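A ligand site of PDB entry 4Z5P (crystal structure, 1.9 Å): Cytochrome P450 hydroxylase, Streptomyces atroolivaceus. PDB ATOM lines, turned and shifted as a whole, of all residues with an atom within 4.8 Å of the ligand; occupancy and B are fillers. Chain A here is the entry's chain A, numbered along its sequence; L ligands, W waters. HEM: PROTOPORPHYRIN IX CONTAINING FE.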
ATOM      1  N   ASN A  59      -8.371   6.975   2.220  1.00  0.00           N
ATOM      2  CA  ASN A  59      -8.194   8.388   2.518  1.00  0.00           C
ATOM      3  C   ASN A  59      -6.788   8.913   2.396  1.00  0.00           C
ATOM      4  O   ASN A  59      -6.591  10.132   2.467  1.00  0.00           O
ATOM      5  CB  ASN A  59      -8.803   8.714   3.882  1.00  0.00           C
ATOM      6  CG  ASN A  59     -10.323   8.591   3.875  1.00  0.00           C
ATOM      7  OD1 ASN A  59     -10.981   8.712   2.824  1.00  0.00           O
ATOM      8  ND2 ASN A  59     -10.891   8.294   5.031  1.00  0.00           N
ATOM      9  N   ARG A  66      -9.336  12.906  -4.895  1.00  0.00           N
ATOM     10  CA  ARG A  66     -10.434  13.734  -4.392  1.00  0.00           C
ATOM     11  C   ARG A  66     -10.957  14.761  -5.403  1.00  0.00           C
ATOM     12  O   ARG A  66     -12.068  15.248  -5.264  1.00  0.00           O
ATOM     13  CB  ARG A  66      -9.941  14.459  -3.154  1.00  0.00           C
ATOM     14  CG  ARG A  66      -9.396  13.489  -2.141  1.00  0.00           C
ATOM     15  CD  ARG A  66      -9.010  14.202  -0.891  1.00  0.00           C
ATOM     16  NE  ARG A  66      -8.484  13.263   0.081  1.00  0.00           N
ATOM     17  CZ  ARG A  66      -8.461  13.468   1.389  1.00  0.00           C
ATOM     18  NH1 ARG A  66      -8.941  14.597   1.910  1.00  0.00           N
ATOM     19  NH2 ARG A  66      -7.951  12.539   2.187  1.00  0.00           N
ATOM     20  N   ILE A  86      -8.576  23.066  -0.506  1.00  0.00           N
ATOM     21  CA  ILE A  86      -7.457  22.142  -0.314  1.00  0.00           C
ATOM     22  C   ILE A  86      -7.915  20.681  -0.051  1.00  0.00           C
ATOM     23  O   ILE A  86      -7.232  19.752  -0.461  1.00  0.00           O
ATOM     24  CB  ILE A  86      -6.505  22.615   0.792  1.00  0.00           C
ATOM     25  CG1 ILE A  86      -5.238  21.751   0.821  1.00  0.00           C
ATOM     26  CG2 ILE A  86      -7.203  22.653   2.134  1.00  0.00           C
ATOM     27  CD1 ILE A  86      -4.110  22.264   1.675  1.00  0.00           C
ATOM     28  N   LEU A  87      -9.018  20.497   0.656  1.00  0.00           N
ATOM     29  CA  LEU A  87      -9.558  19.159   0.953  1.00  0.00           C
ATOM     30  C   LEU A  87      -9.900  18.322  -0.276  1.00  0.00           C
ATOM     31  O   LEU A  87      -9.812  17.078  -0.211  1.00  0.00           O
ATOM     32  CB  LEU A  87     -10.791  19.258   1.849  1.00  0.00           C
ATOM     33  CG  LEU A  87     -10.404  19.618   3.298  1.00  0.00           C
ATOM     34  CD1 LEU A  87     -11.418  20.549   3.951  1.00  0.00           C
ATOM     35  CD2 LEU A  87     -10.174  18.356   4.129  1.00  0.00           C
ATOM     36  N   HIS A  94      -2.106  20.080  -4.654  1.00  0.00           N
ATOM     37  CA  HIS A  94      -2.248  19.976  -3.220  1.00  0.00           C
ATOM     38  C   HIS A  94      -0.927  20.145  -2.503  1.00  0.00           C
ATOM     39  O   HIS A  94      -0.848  20.785  -1.466  1.00  0.00           O
ATOM     40  CB  HIS A  94      -2.836  18.621  -2.820  1.00  0.00           C
ATOM     41  CG  HIS A  94      -2.955  18.464  -1.338  1.00  0.00           C
ATOM     42  ND1 HIS A  94      -2.000  17.791  -0.598  1.00  0.00           N
ATOM     43  CD2 HIS A  94      -3.843  18.963  -0.456  1.00  0.00           C
ATOM     44  CE1 HIS A  94      -2.333  17.861   0.686  1.00  0.00           C
ATOM     45  NE2 HIS A  94      -3.460  18.543   0.787  1.00  0.00           N
ATOM     46  N   ARG A  98      -0.100  22.936   0.279  1.00  0.00           N
ATOM     47  CA  ARG A  98       0.298  22.490   1.602  1.00  0.00           C
ATOM     48  C   ARG A  98       1.707  22.987   2.029  1.00  0.00           C
ATOM     49  O   ARG A  98       1.896  23.314   3.216  1.00  0.00           O
ATOM     50  CB  ARG A  98       0.306  20.972   1.607  1.00  0.00           C
ATOM     51  CG  ARG A  98       0.520  20.343   2.938  1.00  0.00           C
ATOM     52  CD  ARG A  98      -0.782  19.892   3.556  1.00  0.00           C
ATOM     53  NE  ARG A  98      -0.468  19.331   4.860  1.00  0.00           N
ATOM     54  CZ  ARG A  98      -1.347  18.908   5.755  1.00  0.00           C
ATOM     55  NH1 ARG A  98      -2.652  18.902   5.481  1.00  0.00           N
ATOM     56  NH2 ARG A  98      -0.901  18.431   6.898  1.00  0.00           N
ATOM     57  N   PHE A 105       1.432  27.344   9.580  1.00  0.00           N
ATOM     58  CA  PHE A 105       1.016  26.319  10.531  1.00  0.00           C
ATOM     59  C   PHE A 105       2.261  25.551  10.948  1.00  0.00           C
ATOM     60  O   PHE A 105       2.546  24.496  10.385  1.00  0.00           O
ATOM     61  CB  PHE A 105      -0.021  25.377   9.932  1.00  0.00           C
ATOM     62  CG  PHE A 105      -1.355  25.979   9.754  1.00  0.00           C
ATOM     63  CD1 PHE A 105      -1.649  26.737   8.612  1.00  0.00           C
ATOM     64  CD2 PHE A 105      -2.332  25.822  10.719  1.00  0.00           C
ATOM     65  CE1 PHE A 105      -2.910  27.293   8.440  1.00  0.00           C
ATOM     66  CE2 PHE A 105      -3.591  26.396  10.561  1.00  0.00           C
ATOM     67  CZ  PHE A 105      -3.869  27.139   9.429  1.00  0.00           C
ATOM     68  N   ILE A 150     -10.299  30.918  15.680  1.00  0.00           N
ATOM     69  CA  ILE A 150     -10.155  31.108  14.217  1.00  0.00           C
ATOM     70  C   ILE A 150     -10.049  32.624  13.903  1.00  0.00           C
ATOM     71  O   ILE A 150      -9.249  33.035  13.045  1.00  0.00           O
ATOM     72  CB  ILE A 150     -11.278  30.419  13.433  1.00  0.00           C
ATOM     73  CG1 ILE A 150     -11.238  28.909  13.669  1.00  0.00           C
ATOM     74  CG2 ILE A 150     -11.128  30.674  11.948  1.00  0.00           C
ATOM     75  CD1 ILE A 150      -9.893  28.231  13.480  1.00  0.00           C
ATOM     76  N   LEU A 153      -6.555  33.638  14.359  1.00  0.00           N
ATOM     77  CA  LEU A 153      -5.704  33.188  13.221  1.00  0.00           C
ATOM     78  C   LEU A 153      -5.867  34.121  11.990  1.00  0.00           C
ATOM     79  O   LEU A 153      -4.885  34.445  11.324  1.00  0.00           O
ATOM     80  CB  LEU A 153      -5.985  31.760  12.823  1.00  0.00           C
ATOM     81  CG  LEU A 153      -5.799  30.692  13.908  1.00  0.00           C
ATOM     82  CD1 LEU A 153      -6.036  29.306  13.328  1.00  0.00           C
ATOM     83  CD2 LEU A 153      -4.453  30.784  14.618  1.00  0.00           C
ATOM     84  N   PHE A 230      -8.958  29.792   1.364  1.00  0.00           N
ATOM     85  CA  PHE A 230      -8.453  29.139   2.565  1.00  0.00           C
ATOM     86  C   PHE A 230      -9.054  29.702   3.860  1.00  0.00           C
ATOM     87  O   PHE A 230      -9.334  28.923   4.794  1.00  0.00           O
ATOM     88  CB  PHE A 230      -6.945  29.159   2.649  1.00  0.00           C
ATOM     89  CG  PHE A 230      -6.428  28.387   3.805  1.00  0.00           C
ATOM     90  CD1 PHE A 230      -6.492  27.009   3.796  1.00  0.00           C
ATOM     91  CD2 PHE A 230      -5.982  29.024   4.943  1.00  0.00           C
ATOM     92  CE1 PHE A 230      -6.040  26.282   4.887  1.00  0.00           C
ATOM     93  CE2 PHE A 230      -5.526  28.308   6.025  1.00  0.00           C
ATOM     94  CZ  PHE A 230      -5.566  26.929   5.989  1.00  0.00           C
ATOM     95  N   LEU A 234     -10.981  27.549   6.603  1.00  0.00           N
ATOM     96  CA  LEU A 234     -10.597  27.568   7.996  1.00  0.00           C
ATOM     97  C   LEU A 234     -11.813  27.720   8.923  1.00  0.00           C
ATOM     98  O   LEU A 234     -11.794  27.196  10.031  1.00  0.00           O
ATOM     99  CB  LEU A 234      -9.549  28.663   8.219  1.00  0.00           C
ATOM    100  CG  LEU A 234      -8.476  28.598   9.263  1.00  0.00           C
ATOM    101  CD1 LEU A 234      -7.658  27.309   9.195  1.00  0.00           C
ATOM    102  CD2 LEU A 234      -7.586  29.826   9.100  1.00  0.00           C
ATOM    103  N   ALA A 237     -13.389  23.953   8.577  1.00  0.00           N
ATOM    104  CA  ALA A 237     -12.449  22.927   9.095  1.00  0.00           C
ATOM    105  C   ALA A 237     -12.001  23.260  10.509  1.00  0.00           C
ATOM    106  O   ALA A 237     -11.867  22.369  11.332  1.00  0.00           O
ATOM    107  CB  ALA A 237     -11.239  22.813   8.193  1.00  0.00           C
ATOM    108  N   GLY A 238     -11.780  24.549  10.818  1.00  0.00           N
ATOM    109  CA  GLY A 238     -11.267  24.877  12.129  1.00  0.00           C
ATOM    110  C   GLY A 238     -12.271  25.261  13.223  1.00  0.00           C
ATOM    111  O   GLY A 238     -12.009  25.066  14.425  1.00  0.00           O
ATOM    112  N   THR A 241     -15.965  22.333  12.850  1.00  0.00           N
ATOM    113  CA  THR A 241     -15.477  20.999  13.253  1.00  0.00           C
ATOM    114  C   THR A 241     -15.121  20.981  14.718  1.00  0.00           C
ATOM    115  O   THR A 241     -15.657  20.188  15.466  1.00  0.00           O
ATOM    116  CB  THR A 241     -14.312  20.574  12.353  1.00  0.00           C
ATOM    117  OG1 THR A 241     -14.790  20.576  10.999  1.00  0.00           O
ATOM    118  CG2 THR A 241     -13.793  19.195  12.684  1.00  0.00           C
ATOM    119  N   SER A 242     -14.262  21.902  15.153  1.00  0.00           N
ATOM    120  CA  SER A 242     -13.855  21.928  16.540  1.00  0.00           C
ATOM    121  C   SER A 242     -15.011  22.136  17.494  1.00  0.00           C
ATOM    122  O   SER A 242     -15.021  21.500  18.563  1.00  0.00           O
ATOM    123  CB  SER A 242     -12.798  22.994  16.801  1.00  0.00           C
ATOM    124  OG  SER A 242     -11.714  22.838  15.925  1.00  0.00           O
ATOM    125  N   GLN A 245     -17.159  18.876  17.675  1.00  0.00           N
ATOM    126  CA  GLN A 245     -16.383  17.815  18.283  1.00  0.00           C
ATOM    127  C   GLN A 245     -16.302  18.020  19.774  1.00  0.00           C
ATOM    128  O   GLN A 245     -16.385  17.045  20.541  1.00  0.00           O
ATOM    129  CB  GLN A 245     -14.968  17.772  17.659  1.00  0.00           C
ATOM    130  CG  GLN A 245     -14.052  16.728  18.252  1.00  0.00           C
ATOM    131  CD  GLN A 245     -14.436  15.306  17.869  1.00  0.00           C
ATOM    132  OE1 GLN A 245     -14.973  15.059  16.789  1.00  0.00           O
ATOM    133  NE2 GLN A 245     -14.149  14.381  18.722  1.00  0.00           N
ATOM    134  N   LEU A 278     -11.480  11.624  20.762  1.00  0.00           N
ATOM    135  CA  LEU A 278     -11.336  11.755  19.281  1.00  0.00           C
ATOM    136  C   LEU A 278     -11.607  10.444  18.532  1.00  0.00           C
ATOM    137  O   LEU A 278     -12.250  10.423  17.454  1.00  0.00           O
ATOM    138  CB  LEU A 278      -9.926  12.256  18.932  1.00  0.00           C
ATOM    139  CG  LEU A 278      -9.737  13.761  19.213  1.00  0.00           C
ATOM    140  CD1 LEU A 278      -8.300  14.176  19.296  1.00  0.00           C
ATOM    141  CD2 LEU A 278     -10.436  14.553  18.142  1.00  0.00           C
ATOM    142  N   LEU A 283     -18.662  12.307  14.508  1.00  0.00           N
ATOM    143  CA  LEU A 283     -18.747  13.739  14.173  1.00  0.00           C
ATOM    144  C   LEU A 283     -19.724  13.990  13.016  1.00  0.00           C
ATOM    145  O   LEU A 283     -20.592  14.862  13.103  1.00  0.00           O
ATOM    146  CB  LEU A 283     -17.359  14.276  13.815  1.00  0.00           C
ATOM    147  CG  LEU A 283     -17.187  15.798  13.636  1.00  0.00           C
ATOM    148  CD1 LEU A 283     -17.760  16.578  14.832  1.00  0.00           C
ATOM    149  CD2 LEU A 283     -15.724  16.151  13.430  1.00  0.00           C
ATOM    150  N   ARG A 291     -13.879   8.860  -2.857  1.00  0.00           N
ATOM    151  CA  ARG A 291     -12.590   8.988  -3.500  1.00  0.00           C
ATOM    152  C   ARG A 291     -12.693   8.150  -4.751  1.00  0.00           C
ATOM    153  O   ARG A 291     -13.385   7.125  -4.743  1.00  0.00           O
ATOM    154  CB  ARG A 291     -11.462   8.445  -2.622  1.00  0.00           C
ATOM    155  CG  ARG A 291     -11.569   8.729  -1.141  1.00  0.00           C
ATOM    156  CD  ARG A 291     -11.568  10.212  -0.884  1.00  0.00           C
ATOM    157  NE  ARG A 291     -11.407  10.550   0.526  1.00  0.00           N
ATOM    158  CZ  ARG A 291     -11.689  11.744   1.057  1.00  0.00           C
ATOM    159  NH1 ARG A 291     -12.152  12.729   0.295  1.00  0.00           N
ATOM    160  NH2 ARG A 291     -11.511  11.942   2.348  1.00  0.00           N
ATOM    161  N   LEU A 340      -7.883   7.715  13.360  1.00  0.00           N
ATOM    162  CA  LEU A 340      -7.888   8.464  12.120  1.00  0.00           C
ATOM    163  C   LEU A 340      -8.720   9.745  12.124  1.00  0.00           C
ATOM    164  O   LEU A 340      -9.089  10.256  11.069  1.00  0.00           O
ATOM    165  CB  LEU A 340      -8.367   7.533  10.989  1.00  0.00           C
ATOM    166  CG  LEU A 340      -7.562   6.248  10.725  1.00  0.00           C
ATOM    167  CD1 LEU A 340      -8.148   5.460   9.545  1.00  0.00           C
ATOM    168  CD2 LEU A 340      -6.116   6.558  10.428  1.00  0.00           C
ATOM    169  N   ALA A 341      -9.106  10.225  13.299  1.00  0.00           N
ATOM    170  CA  ALA A 341      -9.913  11.434  13.461  1.00  0.00           C
ATOM    171  C   ALA A 341      -9.317  12.698  12.857  1.00  0.00           C
ATOM    172  O   ALA A 341     -10.072  13.588  12.515  1.00  0.00           O
ATOM    173  CB  ALA A 341     -10.214  11.674  14.936  1.00  0.00           C
ATOM    174  N   PHE A 342      -7.988  12.780  12.766  1.00  0.00           N
ATOM    175  CA  PHE A 342      -7.322  13.846  12.024  1.00  0.00           C
ATOM    176  C   PHE A 342      -6.836  13.430  10.659  1.00  0.00           C
ATOM    177  O   PHE A 342      -6.110  14.160  10.015  1.00  0.00           O
ATOM    178  CB  PHE A 342      -6.147  14.392  12.808  1.00  0.00           C
ATOM    179  CG  PHE A 342      -6.539  15.095  14.074  1.00  0.00           C
ATOM    180  CD1 PHE A 342      -7.324  16.230  14.035  1.00  0.00           C
ATOM    181  CD2 PHE A 342      -6.050  14.669  15.292  1.00  0.00           C
ATOM    182  CE1 PHE A 342      -7.646  16.914  15.208  1.00  0.00           C
ATOM    183  CE2 PHE A 342      -6.379  15.315  16.458  1.00  0.00           C
ATOM    184  CZ  PHE A 342      -7.193  16.456  16.416  1.00  0.00           C
ATOM    185  N   GLY A 343      -7.212  12.211  10.232  1.00  0.00           N
ATOM    186  CA  GLY A 343      -6.735  11.632   8.987  1.00  0.00           C
ATOM    187  C   GLY A 343      -5.358  11.027   9.068  1.00  0.00           C
ATOM    188  O   GLY A 343      -4.868  10.717  10.149  1.00  0.00           O
ATOM    189  N   HIS A 344      -4.751  10.866   7.899  1.00  0.00           N
ATOM    190  CA  HIS A 344      -3.465  10.224   7.747  1.00  0.00           C
ATOM    191  C   HIS A 344      -2.877  10.589   6.399  1.00  0.00           C
ATOM    192  O   HIS A 344      -3.572  10.633   5.424  1.00  0.00           O
ATOM    193  CB  HIS A 344      -3.672   8.713   7.830  1.00  0.00           C
ATOM    194  CG  HIS A 344      -2.418   7.930   7.695  1.00  0.00           C
ATOM    195  ND1 HIS A 344      -2.033   7.340   6.504  1.00  0.00           N
ATOM    196  CD2 HIS A 344      -1.430   7.659   8.585  1.00  0.00           C
ATOM    197  CE1 HIS A 344      -0.879   6.721   6.681  1.00  0.00           C
ATOM    198  NE2 HIS A 344      -0.505   6.889   7.928  1.00  0.00           N
ATOM    199  N   ALA A 346      -1.204  12.785   3.313  1.00  0.00           N
ATOM    200  CA  ALA A 346      -1.010  14.119   2.745  1.00  0.00           C
ATOM    201  C   ALA A 346      -1.966  15.202   3.285  1.00  0.00           C
ATOM    202  O   ALA A 346      -1.562  16.353   3.472  1.00  0.00           O
ATOM    203  CB  ALA A 346      -1.113  14.036   1.225  1.00  0.00           C
ATOM    204  N   HIS A 347      -3.211  14.798   3.550  1.00  0.00           N
ATOM    205  CA  HIS A 347      -4.266  15.725   3.962  1.00  0.00           C
ATOM    206  C   HIS A 347      -4.423  15.796   5.478  1.00  0.00           C
ATOM    207  O   HIS A 347      -5.339  16.449   5.957  1.00  0.00           O
ATOM    208  CB  HIS A 347      -5.620  15.346   3.314  1.00  0.00           C
ATOM    209  CG  HIS A 347      -5.723  15.686   1.851  1.00  0.00           C
ATOM    210  ND1 HIS A 347      -6.267  16.865   1.387  1.00  0.00           N
ATOM    211  CD2 HIS A 347      -5.412  14.951   0.752  1.00  0.00           C
ATOM    212  CE1 HIS A 347      -6.276  16.857   0.057  1.00  0.00           C
ATOM    213  NE2 HIS A 347      -5.742  15.710  -0.356  1.00  0.00           N
ATOM    214  N   TYR A 348      -3.541  15.126   6.217  1.00  0.00           N
ATOM    215  CA  TYR A 348      -3.578  15.143   7.674  1.00  0.00           C
ATOM    216  C   TYR A 348      -3.875  16.530   8.239  1.00  0.00           C
ATOM    217  O   TYR A 348      -3.214  17.517   7.864  1.00  0.00           O
ATOM    218  CB  TYR A 348      -2.279  14.619   8.234  1.00  0.00           C
ATOM    219  CG  TYR A 348      -2.263  14.476   9.730  1.00  0.00           C
ATOM    220  CD1 TYR A 348      -2.771  13.331  10.324  1.00  0.00           C
ATOM    221  CD2 TYR A 348      -1.703  15.443  10.541  1.00  0.00           C
ATOM    222  CE1 TYR A 348      -2.771  13.178  11.703  1.00  0.00           C
ATOM    223  CE2 TYR A 348      -1.707  15.288  11.940  1.00  0.00           C
ATOM    224  CZ  TYR A 348      -2.250  14.154  12.509  1.00  0.00           C
ATOM    225  OH  TYR A 348      -2.255  13.973  13.874  1.00  0.00           O
ATOM    226  N   CYS A 349      -4.846  16.608   9.144  1.00  0.00           N
ATOM    227  CA  CYS A 349      -5.326  17.891   9.675  1.00  0.00           C
ATOM    228  C   CYS A 349      -4.176  18.908   9.935  1.00  0.00           C
ATOM    229  O   CYS A 349      -3.312  18.692  10.762  1.00  0.00           O
ATOM    230  CB  CYS A 349      -6.002  17.663  10.976  1.00  0.00           C
ATOM    231  SG  CYS A 349      -6.648  19.170  11.714  1.00  0.00           S
ATOM    232  N   LEU A 350      -4.239  20.014   9.233  1.00  0.00           N
ATOM    233  CA  LEU A 350      -3.188  21.038   9.314  1.00  0.00           C
ATOM    234  C   LEU A 350      -3.209  21.749  10.672  1.00  0.00           C
ATOM    235  O   LEU A 350      -2.212  22.319  11.134  1.00  0.00           O
ATOM    236  CB  LEU A 350      -3.379  21.984   8.162  1.00  0.00           C
ATOM    237  CG  LEU A 350      -2.234  22.855   7.686  1.00  0.00           C
ATOM    238  CD1 LEU A 350      -1.024  22.084   7.209  1.00  0.00           C
ATOM    239  CD2 LEU A 350      -2.788  23.711   6.556  1.00  0.00           C
ATOM    240  N   GLY A 351      -4.349  21.660  11.344  1.00  0.00           N
ATOM    241  CA  GLY A 351      -4.493  22.161  12.674  1.00  0.00           C
ATOM    242  C   GLY A 351      -4.462  21.244  13.835  1.00  0.00           C
ATOM    243  O   GLY A 351      -4.866  21.645  14.946  1.00  0.00           O
ATOM    244  N   LEU A 354      -3.161  22.387  17.323  1.00  0.00           N
ATOM    245  CA  LEU A 354      -4.010  23.414  17.893  1.00  0.00           C
ATOM    246  C   LEU A 354      -5.361  22.839  18.375  1.00  0.00           C
ATOM    247  O   LEU A 354      -5.874  23.186  19.441  1.00  0.00           O
ATOM    248  CB  LEU A 354      -4.208  24.540  16.846  1.00  0.00           C
ATOM    249  CG  LEU A 354      -5.074  25.711  17.310  1.00  0.00           C
ATOM    250  CD1 LEU A 354      -4.571  26.279  18.611  1.00  0.00           C
ATOM    251  CD2 LEU A 354      -5.053  26.763  16.206  1.00  0.00           C
ATOM    252  N   ALA A 355      -5.937  21.954  17.582  1.00  0.00           N
ATOM    253  CA  ALA A 355      -7.176  21.220  17.969  1.00  0.00           C
ATOM    254  C   ALA A 355      -7.009  20.449  19.273  1.00  0.00           C
ATOM    255  O   ALA A 355      -7.818  20.567  20.189  1.00  0.00           O
ATOM    256  CB  ALA A 355      -7.587  20.239  16.873  1.00  0.00           C
ATOM    257  N   GLU A 358      -6.790  22.953  22.061  1.00  0.00           N
ATOM    258  CA  GLU A 358      -8.157  23.428  22.321  1.00  0.00           C
ATOM    259  C   GLU A 358      -8.999  22.463  23.150  1.00  0.00           C
ATOM    260  O   GLU A 358      -9.691  22.870  24.113  1.00  0.00           O
ATOM    261  CB  GLU A 358      -8.926  23.694  21.016  1.00  0.00           C
ATOM    262  CG  GLU A 358      -8.491  24.897  20.214  1.00  0.00           C
ATOM    263  CD  GLU A 358      -9.346  25.079  18.955  1.00  0.00           C
ATOM    264  OE1 GLU A 358     -10.064  24.166  18.564  1.00  0.00           O
ATOM    265  OE2 GLU A 358      -9.225  26.119  18.315  1.00  0.00           O
ATOM    266  N   LEU A 359      -8.941  21.192  22.787  1.00  0.00           N
ATOM    267  CA  LEU A 359      -9.752  20.183  23.472  1.00  0.00           C
ATOM    268  C   LEU A 359      -9.221  19.942  24.895  1.00  0.00           C
ATOM    269  O   LEU A 359     -10.006  19.830  25.806  1.00  0.00           O
ATOM    270  CB  LEU A 359      -9.822  18.904  22.668  1.00  0.00           C
ATOM    271  CG  LEU A 359     -10.421  18.972  21.242  1.00  0.00           C
ATOM    272  CD1 LEU A 359     -10.225  17.606  20.541  1.00  0.00           C
ATOM    273  CD2 LEU A 359     -11.866  19.349  21.313  1.00  0.00           C
HETATM  274  CHA HEM L   1      -8.293  18.562   7.567  1.00  0.00           C
HETATM  275  CHB HEM L   1     -10.250  16.759  11.547  1.00  0.00           C
HETATM  276  CHC HEM L   1      -9.530  21.007  13.738  1.00  0.00           C
HETATM  277  CHD HEM L   1      -7.430  22.785   9.808  1.00  0.00           C
HETATM  278  C1A HEM L   1      -8.862  17.709   8.465  1.00  0.00           C
HETATM  279  C2A HEM L   1      -9.272  16.386   8.203  1.00  0.00           C
HETATM  280  C3A HEM L   1      -9.831  15.867   9.321  1.00  0.00           C
HETATM  281  C4A HEM L   1      -9.744  16.889  10.287  1.00  0.00           C
HETATM  282  CMA HEM L   1     -10.409  14.464   9.491  1.00  0.00           C
HETATM  283  CAA HEM L   1      -9.191  15.647   6.892  1.00  0.00           C
HETATM  284  CBA HEM L   1      -8.106  14.612   6.850  1.00  0.00           C
HETATM  285  CGA HEM L   1      -8.227  13.977   5.448  1.00  0.00           C
HETATM  286  O1A HEM L   1      -7.437  13.129   5.056  1.00  0.00           O
HETATM  287  O2A HEM L   1      -9.120  14.311   4.633  1.00  0.00           O
HETATM  288  C1B HEM L   1     -10.298  17.758  12.489  1.00  0.00           C
HETATM  289  C2B HEM L   1     -10.830  17.584  13.799  1.00  0.00           C
HETATM  290  C3B HEM L   1     -10.644  18.816  14.432  1.00  0.00           C
HETATM  291  C4B HEM L   1      -9.938  19.685  13.466  1.00  0.00           C
HETATM  292  CMB HEM L   1     -11.541  16.355  14.390  1.00  0.00           C
HETATM  293  CAB HEM L   1     -10.974  19.329  15.785  1.00  0.00           C
HETATM  294  CBB HEM L   1     -11.409  18.656  16.810  1.00  0.00           C
HETATM  295  C1C HEM L   1      -8.876  21.863  12.905  1.00  0.00           C
HETATM  296  C2C HEM L   1      -8.354  23.148  13.272  1.00  0.00           C
HETATM  297  C3C HEM L   1      -7.769  23.677  12.129  1.00  0.00           C
HETATM  298  C4C HEM L   1      -7.901  22.686  11.087  1.00  0.00           C
HETATM  299  CMC HEM L   1      -8.453  23.780  14.627  1.00  0.00           C
HETATM  300  CAC HEM L   1      -7.049  24.970  11.957  1.00  0.00           C
HETATM  301  CBC HEM L   1      -6.788  25.879  12.906  1.00  0.00           C
HETATM  302  C1D HEM L   1      -7.542  21.737   8.905  1.00  0.00           C
HETATM  303  C2D HEM L   1      -7.117  21.935   7.509  1.00  0.00           C
HETATM  304  C3D HEM L   1      -7.333  20.768   6.890  1.00  0.00           C
HETATM  305  C4D HEM L   1      -7.938  19.863   7.898  1.00  0.00           C
HETATM  306  CMD HEM L   1      -6.482  23.174   6.887  1.00  0.00           C
HETATM  307  CAD HEM L   1      -7.053  20.479   5.426  1.00  0.00           C
HETATM  308  CBD HEM L   1      -5.661  19.858   5.212  1.00  0.00           C
HETATM  309  CGD HEM L   1      -5.531  19.247   3.814  1.00  0.00           C
HETATM  310  O1D HEM L   1      -4.389  19.069   3.322  1.00  0.00           O
HETATM  311  O2D HEM L   1      -6.509  18.959   3.117  1.00  0.00           O
HETATM  312  NA  HEM L   1      -9.122  17.989   9.768  1.00  0.00           N
HETATM  313  NB  HEM L   1      -9.737  18.970  12.372  1.00  0.00           N
HETATM  314  NC  HEM L   1      -8.537  21.585  11.625  1.00  0.00           N
HETATM  315  ND  HEM L   1      -7.985  20.465   9.125  1.00  0.00           N
HETATM  316 FE   HEM L   1      -8.792  19.735  10.685  1.00  0.00          FE
HETATM  317  O   HOH W   1     -11.003  20.181  10.274  1.00  0.00           O
HETATM  318  O   HOH W   2      -4.571  12.283   3.488  1.00  0.00           O
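The backbone carbonyl oxygen (O) of Ala 237 lies close to a nitrogen (NC) of the ligand (3.4 Å). Ile 86 touches the ligand (CD1 to O1D, 3.6 Å). Leu 87 touches the ligand (CA to O2D, 3.7 Å). Phe 105 touches the ligand. Ile 150 touches the ligand (CD1 to CBC, 3.9 Å). CD1 of Leu 153 touches CBC of the ligand (3.5 Å). Phe 230 touches the ligand (CE1 to CMD, 3.7 Å). Leu 234 touches the ligand (CD1 to CAC, 3.7 Å). Gly 238 touches the ligand. Thr 241 touches the ligand (CG2 to C2B, 3.6 Å). Ser 242 touches the ligand. CG of Gln 245 touches CBB of the ligand (3.6 Å). Ala 341 touches the ligand (O to CMA, 3.2 Å). Phe 342 touches the ligand. Gly 343 touches the ligand (CA to CBA, 3.9 Å). Ala 346 touches the ligand. Leu 350 touches the ligand (CB to CMD, 3.6 Å). Gly 351 touches the ligand. Leu 354 touches the ligand. Ala 355 touches the ligand. Hydrophobic or aromatic side chains within 4 Å of the ligand: Ile 86, Leu 87, His 94, Phe 105, Ile 150, Leu 153, Phe 230, Leu 234, Ala 237, Phe 342, His 347, Leu 350, Leu 354 and Ala 355. Within 4 Å of the ligand: Arg 66, Ile 86, Leu 87, His 94, Arg 98, Phe 105, Ile 150, Leu 153, Phe 230, Leu 234, Ala 237, Gly 238, Thr 241, Ser 242, Gln 245, Ala 341, Phe 342, Gly 343, Ala 346, His 347, Cys 349, Leu 350, Gly 351, Leu 354 and Ala 355. The nearest printed residue that does not touch the ligand is Asn 59 (4.05 Å).
The side-chain sulfur (SG) of Cys 349 sits close to the backbone NH (N) of Gly 351. ND1 of His 347 is in hydrogen-bond range of NE2 of His 94 (3.3 Å). The guanidinium group of Arg 66 lies close to the backbone carbonyl oxygen of Leu 87 (3.4 Å). The guanidinium group (NH2) of Arg 66 sits at hydrogen-bond distance from the backbone carbonyl oxygen (O) of Asn 59 (2.8 Å). The guanidinium group (NH2) of Arg 98 sits at hydrogen-bond distance from the backbone carbonyl oxygen (O) of Tyr 348, 2.7 Å away. The backbone carbonyl oxygen (O) of Ala 237 lies close to the side-chain hydroxyl (OG1) of Thr 241, at 3.4 Å. O of Gly 238 is in hydrogen-bond range of OG of Ser 242 (2.7 Å). The side-chain carboxylate (OE1) of Glu 358 lies within hydrogen-bond range of the side-chain hydroxyl (OG) of Ser 242.
The side-chain sulfur (SG) of Cys 349 binds an iron atom (FE) of the ligand (2.4 Å). An oxygen (O2D) of the ligand sits at hydrogen-bond distance from a ring nitrogen (ND1) of His 347, 2.7 Å away. An oxygen (O2A) of the ligand lies within salt-bridge range of the guanidinium group of Arg 66 (2.7 Å). NE2 of His 94 is in hydrogen-bond range of O1D of the ligand. The guanidinium group (NH1) of Arg 98 lies within salt-bridge range of an oxygen (O1D) of the ligand (2.8 Å).
Water W2 lies within hydrogen-bond range of O of His 344 (2.7 Å), N of His 347 (2.9 Å), O of Asn 59 (3.1 Å), O1A of the ligand (3.4 Å) and N of Ala 346 (3.4 Å).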
